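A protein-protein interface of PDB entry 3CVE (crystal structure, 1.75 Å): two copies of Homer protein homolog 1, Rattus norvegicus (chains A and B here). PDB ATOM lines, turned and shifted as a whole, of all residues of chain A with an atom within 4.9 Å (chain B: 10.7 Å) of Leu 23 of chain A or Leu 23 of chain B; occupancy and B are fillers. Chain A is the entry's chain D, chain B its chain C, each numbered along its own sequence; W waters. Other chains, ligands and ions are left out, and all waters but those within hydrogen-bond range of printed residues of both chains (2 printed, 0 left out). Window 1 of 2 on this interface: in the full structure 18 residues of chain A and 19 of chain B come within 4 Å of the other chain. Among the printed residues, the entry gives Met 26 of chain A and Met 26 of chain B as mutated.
The side-chain carboxylate of Asp 18 of chain B is in salt-bridge range of the guanidinium group of Arg 15 of chain B (3.8 Å). The side-chain amide nitrogen of Gln 22 of chain B sits at hydrogen-bond distance from the side-chain carboxylate of Asp 18 of chain B (3.1 Å).
Of the 17 printed residues of chain B, 8 touch a printed residue of chain A. Hydrophobic or aromatic side chains of chain B within 4 Å of the printed part of chain A: Leu 19, Leu 23, Met 26 and Leu 30. Of the 9 printed residues of chain A, 6 touch a printed residue of chain B. Hydrophobic or aromatic side chains of chain A that line the printed part of chain B: Leu 19, Leu 23 and Met 26. Along chain A the printed residues that touch a printed residue of chain B span positions 19 to 27. Among the printed residues, 12 pairs touch across the chains.
Water W2 lies within hydrogen-bond range of the side-chain carboxylate (OE2) of Glu 20 of chain A and the guanidinium group (NE) of Arg 15 of chain B. Water W1 lies within hydrogen-bond range of OE1 of Gln 22 of chain A (3.0 Å) and OE2 of Glu 27 of chain B (3.1 Å).
Glu 20 of chain A touches Leu 19 of chain B, but with the chains exchanged Leu 19 of chain A does not touch Glu 20 of chain B (4.2 Å). Gln 22 of chain A touches Leu 23 of chain B, and with the chains exchanged Leu 23 of chain A touches Gln 22 of chain B. Leu 23 of chain A touches Leu 19 of chain B, but with the chains exchanged Leu 19 of chain A does not touch Leu 23 of chain B (4.4 Å). Leu 23 of chain B touches its own counterpart, Leu 23 of chain A. Positions printed for both chains: 19, 20, 21, 22, 23, 24, 25, 26 and 27. Of the 12 pairs that touch across the chains among the printed residues, 6 have their exchanged pair printed and touching as well.
The guanidinium group of Arg 15 of chain B is in salt-bridge range of the side-chain carboxylate of Glu 20 of chain A, 2.7 Å away.
Gly 21 of chain A touches none of the printed residues of chain B. Gln 22 of chain A touches just one residue of chain B: Leu 23. Leu 23 of chain A touches three residues of chain B. No residue of chain B comes within 4 Å of Ser 24 of chain A. Of chain B, only Leu 23 (3.8 Å), Met 26 (3.6 Å), Glu 27 (3.9 Å) and Leu 30 (3.3 Å) come within 4 Å of Met 26 of chain A. Of chain B, only Met 26 (3.0 Å) comes within 4 Å of Glu 27 of chain A. Printed residues of chain A within 4 Å of Arg 15 of chain B: Glu 20 (2.7 Å). Of the printed residues of chain A, Asn 16 of chain B touches Leu 19 (3.7 Å). Of chain A, only Gln 22, Leu 23 and Met 26 come within 4 Å of Leu 23 of chain B. Glu 25 of chain B touches none of the printed residues of chain A. The nearest residue of chain A that does not touch Leu 23 of chain B is Leu 19 of chain A (4.4 Å).
Among the printed residues, merely in contact across the chains: Leu 19 of chain A with Asn 16 of chain B, Glu 20 of chain A with Leu 19 of chain B, Gln 22 of chain A with Leu 23 of chain B, Leu 23 of chain A with Leu 19 of chain B, Leu 23 of chain A with Gln 22 of chain B, Leu 23 of chain A with Leu 23 of chain B, Met 26 of chain A with Leu 23 of chain B, Met 26 of chain A with Met 26 of chain B, Met 26 of chain A with Glu 27 of chain B, Met 26 of chain A with Leu 30 of chain B and Glu 27 of chain A with Met 26 of chain B.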
ATOM      1  N   LEU A  19      12.561 -13.624 -29.132  1.00  0.00           N
ATOM      2  CA  LEU A  19      12.542 -14.910 -28.424  1.00  0.00           C
ATOM      3  C   LEU A  19      11.203 -15.624 -28.557  1.00  0.00           C
ATOM      4  O   LEU A  19      11.158 -16.812 -28.842  1.00  0.00           O
ATOM      5  CB  LEU A  19      12.875 -14.738 -26.932  1.00  0.00           C
ATOM      6  CG  LEU A  19      14.351 -14.452 -26.645  1.00  0.00           C
ATOM      7  CD1 LEU A  19      14.474 -13.985 -25.207  1.00  0.00           C
ATOM      8  CD2 LEU A  19      15.225 -15.712 -26.912  1.00  0.00           C
ATOM      9  N   GLU A  20      10.113 -14.890 -28.370  1.00  0.00           N
ATOM     10  CA  GLU A  20       8.782 -15.441 -28.610  1.00  0.00           C
ATOM     11  C   GLU A  20       8.604 -16.012 -30.033  1.00  0.00           C
ATOM     12  O   GLU A  20       7.978 -17.063 -30.203  1.00  0.00           O
ATOM     13  CB  GLU A  20       7.685 -14.428 -28.263  1.00  0.00           C
ATOM     14  CG  GLU A  20       7.377 -14.269 -26.745  1.00  0.00           C
ATOM     15  CD  GLU A  20       6.649 -15.463 -26.072  1.00  0.00           C
ATOM     16  OE1 GLU A  20       6.474 -16.559 -26.672  1.00  0.00           O
ATOM     17  OE2 GLU A  20       6.236 -15.304 -24.895  1.00  0.00           O
ATOM     18  N   GLY A  21       9.128 -15.303 -31.032  1.00  0.00           N
ATOM     19  CA  GLY A  21       9.104 -15.723 -32.447  1.00  0.00           C
ATOM     20  C   GLY A  21       9.886 -17.009 -32.676  1.00  0.00           C
ATOM     21  O   GLY A  21       9.425 -17.923 -33.383  1.00  0.00           O
ATOM     22  N   GLN A  22      11.051 -17.093 -32.041  1.00  0.00           N
ATOM     23  CA  GLN A  22      11.913 -18.271 -32.121  1.00  0.00           C
ATOM     24  C   GLN A  22      11.302 -19.455 -31.415  1.00  0.00           C
ATOM     25  O   GLN A  22      11.364 -20.586 -31.915  1.00  0.00           O
ATOM     26  CB  GLN A  22      13.247 -17.983 -31.457  1.00  0.00           C
ATOM     27  CG  GLN A  22      14.173 -17.127 -32.282  1.00  0.00           C
ATOM     28  CD  GLN A  22      15.520 -16.983 -31.623  1.00  0.00           C
ATOM     29  OE1 GLN A  22      16.190 -17.977 -31.335  1.00  0.00           O
ATOM     30  NE2 GLN A  22      15.941 -15.744 -31.403  1.00  0.00           N
ATOM     31  N   LEU A  23      10.717 -19.207 -30.247  1.00  0.00           N
ATOM     32  CA  LEU A  23      10.043 -20.282 -29.532  1.00  0.00           C
ATOM     33  C   LEU A  23       8.837 -20.815 -30.333  1.00  0.00           C
ATOM     34  O   LEU A  23       8.620 -22.045 -30.410  1.00  0.00           O
ATOM     35  CB  LEU A  23       9.642 -19.846 -28.108  1.00  0.00           C
ATOM     36  CG  LEU A  23       9.212 -20.969 -27.170  1.00  0.00           C
ATOM     37  CD1 LEU A  23      10.350 -21.954 -26.907  1.00  0.00           C
ATOM     38  CD2 LEU A  23       8.647 -20.417 -25.833  1.00  0.00           C
ATOM     39  N   SER A  24       8.082 -19.904 -30.960  1.00  0.00           N
ATOM     40  CA  SER A  24       6.912 -20.288 -31.787  1.00  0.00           C
ATOM     41  C   SER A  24       7.347 -21.163 -32.972  1.00  0.00           C
ATOM     42  O   SER A  24       6.687 -22.175 -33.307  1.00  0.00           O
ATOM     43  CB  SER A  24       6.172 -19.040 -32.285  1.00  0.00           C
ATOM     44  OG  SER A  24       5.139 -19.358 -33.234  1.00  0.00           O
ATOM     45  N   GLU A  25       8.460 -20.782 -33.596  1.00  0.00           N
ATOM     46  CA  GLU A  25       8.984 -21.564 -34.704  1.00  0.00           C
ATOM     47  C   GLU A  25       9.421 -22.947 -34.224  1.00  0.00           C
ATOM     48  O   GLU A  25       9.088 -23.965 -34.845  1.00  0.00           O
ATOM     49  CB  GLU A  25      10.097 -20.849 -35.469  1.00  0.00           C
ATOM     50  CG  GLU A  25      10.441 -21.566 -36.774  1.00  0.00           C
ATOM     51  CD  GLU A  25       9.224 -21.775 -37.679  1.00  0.00           C
ATOM     52  OE1 GLU A  25       8.550 -20.774 -38.031  1.00  0.00           O
ATOM     53  OE2 GLU A  25       8.936 -22.945 -38.042  1.00  0.00           O
ATOM     54  N   MET A  26      10.103 -22.992 -33.088  1.00  0.00           N
ATOM     55  CA  MET A  26      10.508 -24.284 -32.524  1.00  0.00           C
ATOM     56  C   MET A  26       9.338 -25.200 -32.127  1.00  0.00           C
ATOM     57  O   MET A  26       9.382 -26.424 -32.411  1.00  0.00           O
ATOM     58  CB  MET A  26      11.522 -24.068 -31.401  1.00  0.00           C
ATOM     59  CG  MET A  26      12.905 -23.935 -31.987  1.00  0.00           C
ATOM     60  SD  MET A  26      13.750 -25.645 -32.416  1.00  0.00           S
ATOM     61  CE  MET A  26      12.307 -26.929 -32.145  1.00  0.00           C
ATOM     62  N   GLU A  27       8.282 -24.622 -31.528  1.00  0.00           N
ATOM     63  CA  GLU A  27       7.022 -25.341 -31.263  1.00  0.00           C
ATOM     64  C   GLU A  27       6.515 -25.973 -32.546  1.00  0.00           C
ATOM     65  O   GLU A  27       6.178 -27.158 -32.578  1.00  0.00           O
ATOM     66  CB  GLU A  27       5.914 -24.423 -30.711  1.00  0.00           C
ATOM     67  CG  GLU A  27       6.234 -23.682 -29.425  1.00  0.00           C
ATOM     68  CD  GLU A  27       5.235 -22.568 -29.122  1.00  0.00           C
ATOM     69  OE1 GLU A  27       4.014 -22.817 -29.167  1.00  0.00           O
ATOM     70  OE2 GLU A  27       5.676 -21.450 -28.815  1.00  0.00           O
ATOM     71  N   ARG B  15      11.079 -12.407 -17.936  1.00  0.00           N
ATOM     72  CA  ARG B  15      10.387 -13.200 -18.951  1.00  0.00           C
ATOM     73  C   ARG B  15      11.399 -13.727 -19.952  1.00  0.00           C
ATOM     74  O   ARG B  15      11.354 -14.894 -20.313  1.00  0.00           O
ATOM     75  CB  ARG B  15       9.341 -12.349 -19.693  1.00  0.00           C
ATOM     76  CG  ARG B  15       8.681 -13.090 -20.863  1.00  0.00           C
ATOM     77  CD  ARG B  15       7.905 -14.344 -20.424  1.00  0.00           C
ATOM     78  NE  ARG B  15       7.058 -14.847 -21.503  1.00  0.00           N
ATOM     79  CZ  ARG B  15       6.416 -16.009 -21.463  1.00  0.00           C
ATOM     80  NH1 ARG B  15       6.514 -16.793 -20.384  1.00  0.00           N
ATOM     81  NH2 ARG B  15       5.666 -16.383 -22.498  1.00  0.00           N
ATOM     82  N   ASN B  16      12.303 -12.843 -20.393  1.00  0.00           N
ATOM     83  CA  ASN B  16      13.279 -13.190 -21.423  1.00  0.00           C
ATOM     84  C   ASN B  16      14.225 -14.282 -20.958  1.00  0.00           C
ATOM     85  O   ASN B  16      14.544 -15.176 -21.731  1.00  0.00           O
ATOM     86  CB  ASN B  16      14.073 -11.969 -21.893  1.00  0.00           C
ATOM     87  CG  ASN B  16      13.243 -11.015 -22.764  1.00  0.00           C
ATOM     88  OD1 ASN B  16      12.164 -11.358 -23.241  1.00  0.00           O
ATOM     89  ND2 ASN B  16      13.743  -9.815 -22.944  1.00  0.00           N
ATOM     90  N   LYS B  17      14.661 -14.227 -19.702  1.00  0.00           N
ATOM     91  CA  LYS B  17      15.484 -15.319 -19.159  1.00  0.00           C
ATOM     92  C   LYS B  17      14.748 -16.655 -19.193  1.00  0.00           C
ATOM     93  O   LYS B  17      15.361 -17.680 -19.484  1.00  0.00           O
ATOM     94  CB  LYS B  17      15.958 -15.024 -17.746  1.00  0.00           C
ATOM     95  CG  LYS B  17      16.844 -13.799 -17.660  1.00  0.00           C
ATOM     96  CD  LYS B  17      17.142 -13.456 -16.206  1.00  0.00           C
ATOM     97  CE  LYS B  17      15.882 -12.992 -15.480  1.00  0.00           C
ATOM     98  NZ  LYS B  17      15.631 -13.773 -14.243  1.00  0.00           N
ATOM     99  N   ASP B  18      13.448 -16.651 -18.883  1.00  0.00           N
ATOM    100  CA  ASP B  18      12.625 -17.869 -18.953  1.00  0.00           C
ATOM    101  C   ASP B  18      12.605 -18.372 -20.400  1.00  0.00           C
ATOM    102  O   ASP B  18      12.923 -19.532 -20.689  1.00  0.00           O
ATOM    103  CB  ASP B  18      11.194 -17.565 -18.465  1.00  0.00           C
ATOM    104  CG  ASP B  18      10.288 -18.801 -18.392  1.00  0.00           C
ATOM    105  OD1 ASP B  18      10.770 -19.964 -18.455  1.00  0.00           O
ATOM    106  OD2 ASP B  18       9.058 -18.591 -18.241  1.00  0.00           O
ATOM    107  N   LEU B  19      12.236 -17.478 -21.300  1.00  0.00           N
ATOM    108  CA  LEU B  19      12.142 -17.801 -22.714  1.00  0.00           C
ATOM    109  C   LEU B  19      13.440 -18.428 -23.257  1.00  0.00           C
ATOM    110  O   LEU B  19      13.371 -19.401 -24.013  1.00  0.00           O
ATOM    111  CB  LEU B  19      11.723 -16.571 -23.513  1.00  0.00           C
ATOM    112  CG  LEU B  19      10.259 -16.129 -23.343  1.00  0.00           C
ATOM    113  CD1 LEU B  19       9.997 -14.802 -24.062  1.00  0.00           C
ATOM    114  CD2 LEU B  19       9.262 -17.185 -23.859  1.00  0.00           C
ATOM    115  N   GLU B  20      14.598 -17.894 -22.857  1.00  0.00           N
ATOM    116  CA  GLU B  20      15.895 -18.452 -23.251  1.00  0.00           C
ATOM    117  C   GLU B  20      16.010 -19.939 -22.887  1.00  0.00           C
ATOM    118  O   GLU B  20      16.443 -20.758 -23.709  1.00  0.00           O
ATOM    119  CB  GLU B  20      17.043 -17.678 -22.598  1.00  0.00           C
ATOM    120  CG  GLU B  20      17.341 -16.350 -23.228  1.00  0.00           C
ATOM    121  CD  GLU B  20      18.375 -15.557 -22.434  1.00  0.00           C
ATOM    122  OE1 GLU B  20      19.564 -15.939 -22.411  1.00  0.00           O
ATOM    123  OE2 GLU B  20      18.004 -14.530 -21.842  1.00  0.00           O
ATOM    124  N   GLY B  21      15.617 -20.280 -21.659  1.00  0.00           N
ATOM    125  CA  GLY B  21      15.631 -21.663 -21.198  1.00  0.00           C
ATOM    126  C   GLY B  21      14.601 -22.561 -21.861  1.00  0.00           C
ATOM    127  O   GLY B  21      14.854 -23.751 -22.099  1.00  0.00           O
ATOM    128  N   GLN B  22      13.427 -22.008 -22.140  1.00  0.00           N
ATOM    129  CA  GLN B  22      12.426 -22.757 -22.884  1.00  0.00           C
ATOM    130  C   GLN B  22      12.942 -23.072 -24.275  1.00  0.00           C
ATOM    131  O   GLN B  22      12.805 -24.202 -24.740  1.00  0.00           O
ATOM    132  CB  GLN B  22      11.108 -22.003 -22.952  1.00  0.00           C
ATOM    133  CG  GLN B  22      10.577 -21.638 -21.574  1.00  0.00           C
ATOM    134  CD  GLN B  22       9.097 -21.369 -21.568  1.00  0.00           C
ATOM    135  OE1 GLN B  22       8.327 -22.000 -22.300  1.00  0.00           O
ATOM    136  NE2 GLN B  22       8.677 -20.451 -20.715  1.00  0.00           N
ATOM    137  N   LEU B  23      13.593 -22.097 -24.910  1.00  0.00           N
ATOM    138  CA  LEU B  23      14.052 -22.303 -26.281  1.00  0.00           C
ATOM    139  C   LEU B  23      15.158 -23.363 -26.328  1.00  0.00           C
ATOM    140  O   LEU B  23      15.103 -24.264 -27.160  1.00  0.00           O
ATOM    141  CB  LEU B  23      14.475 -20.982 -26.932  1.00  0.00           C
ATOM    142  CG  LEU B  23      14.979 -21.033 -28.370  1.00  0.00           C
ATOM    143  CD1 LEU B  23      13.856 -21.480 -29.291  1.00  0.00           C
ATOM    144  CD2 LEU B  23      15.495 -19.676 -28.782  1.00  0.00           C
ATOM    145  N   SER B  24      16.119 -23.278 -25.407  1.00  0.00           N
ATOM    146  CA  SER B  24      17.204 -24.259 -25.307  1.00  0.00           C
ATOM    147  C   SER B  24      16.646 -25.673 -25.147  1.00  0.00           C
ATOM    148  O   SER B  24      17.075 -26.603 -25.850  1.00  0.00           O
ATOM    149  CB  SER B  24      18.144 -23.935 -24.137  1.00  0.00           C
ATOM    150  OG  SER B  24      19.059 -25.010 -23.926  1.00  0.00           O
ATOM    151  N   GLU B  25      15.685 -25.821 -24.232  1.00  0.00           N
ATOM    152  CA  GLU B  25      15.046 -27.109 -23.967  1.00  0.00           C
ATOM    153  C   GLU B  25      14.275 -27.601 -25.196  1.00  0.00           C
ATOM    154  O   GLU B  25      14.363 -28.765 -25.557  1.00  0.00           O
ATOM    155  CB  GLU B  25      14.131 -27.006 -22.738  1.00  0.00           C
ATOM    156  CG  GLU B  25      13.016 -28.066 -22.657  1.00  0.00           C
ATOM    157  CD  GLU B  25      13.433 -29.387 -22.029  1.00  0.00           C
ATOM    158  OE1 GLU B  25      12.528 -30.213 -21.748  1.00  0.00           O
ATOM    159  OE2 GLU B  25      14.647 -29.622 -21.816  1.00  0.00           O
ATOM    160  N   MET B  26      13.553 -26.697 -25.850  1.00  0.00           N
ATOM    161  CA  MET B  26      12.819 -27.053 -27.055  1.00  0.00           C
ATOM    162  C   MET B  26      13.736 -27.607 -28.138  1.00  0.00           C
ATOM    163  O   MET B  26      13.461 -28.649 -28.718  1.00  0.00           O
ATOM    164  CB  MET B  26      12.020 -25.865 -27.582  1.00  0.00           C
ATOM    165  CG  MET B  26      10.904 -26.254 -28.512  1.00  0.00           C
ATOM    166  SD  MET B  26       9.396 -27.146 -27.624  1.00  0.00           S
ATOM    167  CE  MET B  26       8.140 -27.115 -29.100  1.00  0.00           C
ATOM    168  N   GLU B  27      14.831 -26.897 -28.385  1.00  0.00           N
ATOM    169  CA  GLU B  27      15.855 -27.288 -29.354  1.00  0.00           C
ATOM    170  C   GLU B  27      16.407 -28.695 -29.027  1.00  0.00           C
ATOM    171  O   GLU B  27      16.497 -29.565 -29.910  1.00  0.00           O
ATOM    172  CB  GLU B  27      16.946 -26.195 -29.394  1.00  0.00           C
ATOM    173  CG  GLU B  27      16.370 -24.768 -29.725  1.00  0.00           C
ATOM    174  CD  GLU B  27      17.389 -23.612 -29.657  1.00  0.00           C
ATOM    175  OE1 GLU B  27      18.316 -23.655 -28.823  1.00  0.00           O
ATOM    176  OE2 GLU B  27      17.246 -22.643 -30.442  1.00  0.00           O
ATOM    177  N   GLN B  28      16.735 -28.919 -27.753  1.00  0.00           N
ATOM    178  CA  GLN B  28      17.164 -30.231 -27.249  1.00  0.00           C
ATOM    179  C   GLN B  28      16.110 -31.334 -27.439  1.00  0.00           C
ATOM    180  O   GLN B  28      16.430 -32.448 -27.835  1.00  0.00           O
ATOM    181  CB  GLN B  28      17.564 -30.124 -25.777  1.00  0.00           C
ATOM    182  CG  GLN B  28      18.951 -29.514 -25.580  1.00  0.00           C
ATOM    183  CD  GLN B  28      19.302 -29.292 -24.126  1.00  0.00           C
ATOM    184  OE1 GLN B  28      18.866 -28.318 -23.510  1.00  0.00           O
ATOM    185  NE2 GLN B  28      20.132 -30.168 -23.579  1.00  0.00           N
ATOM    186  N   ARG B  29      14.856 -31.005 -27.155  1.00  0.00           N
ATOM    187  CA  ARG B  29      13.733 -31.897 -27.417  1.00  0.00           C
ATOM    188  C   ARG B  29      13.686 -32.315 -28.893  1.00  0.00           C
ATOM    189  O   ARG B  29      13.574 -33.503 -29.187  1.00  0.00           O
ATOM    190  CB  ARG B  29      12.406 -31.222 -27.000  1.00  0.00           C
ATOM    191  CG  ARG B  29      11.223 -32.160 -26.923  1.00  0.00           C
ATOM    192  CD  ARG B  29       9.942 -31.477 -26.403  1.00  0.00           C
ATOM    193  NE  ARG B  29      10.005 -31.127 -24.985  1.00  0.00           N
ATOM    194  CZ  ARG B  29       9.624 -31.931 -23.994  1.00  0.00           C
ATOM    195  NH1 ARG B  29       9.145 -33.135 -24.253  1.00  0.00           N
ATOM    196  NH2 ARG B  29       9.709 -31.517 -22.736  1.00  0.00           N
ATOM    197  N   LEU B  30      13.774 -31.349 -29.810  1.00  0.00           N
ATOM    198  CA  LEU B  30      13.720 -31.637 -31.264  1.00  0.00           C
ATOM    199  C   LEU B  30      14.889 -32.523 -31.728  1.00  0.00           C
ATOM    200  O   LEU B  30      14.714 -33.497 -32.475  1.00  0.00           O
ATOM    201  CB  LEU B  30      13.663 -30.323 -32.076  1.00  0.00           C
ATOM    202  CG  LEU B  30      13.556 -30.431 -33.608  1.00  0.00           C
ATOM    203  CD1 LEU B  30      12.233 -31.054 -34.034  1.00  0.00           C
ATOM    204  CD2 LEU B  30      13.715 -29.068 -34.256  1.00  0.00           C
ATOM    205  N   GLU B  31      16.086 -32.185 -31.268  1.00  0.00           N
ATOM    206  CA  GLU B  31      17.285 -32.956 -31.594  1.00  0.00           C
ATOM    207  C   GLU B  31      17.168 -34.406 -31.121  1.00  0.00           C
ATOM    208  O   GLU B  31      17.473 -35.341 -31.873  1.00  0.00           O
ATOM    209  CB  GLU B  31      18.512 -32.282 -30.977  1.00  0.00           C
ATOM    210  CG  GLU B  31      18.733 -30.850 -31.475  1.00  0.00           C
ATOM    211  CD  GLU B  31      20.054 -30.242 -31.028  1.00  0.00           C
ATOM    212  OE1 GLU B  31      20.527 -30.551 -29.902  1.00  0.00           O
ATOM    213  OE2 GLU B  31      20.625 -29.440 -31.810  1.00  0.00           O
HETATM  214  O   HOH W   1      15.902 -20.684 -32.482  1.00  0.00           O
HETATM  215  O   HOH W   2       6.467 -12.840 -23.567  1.00  0.00           O
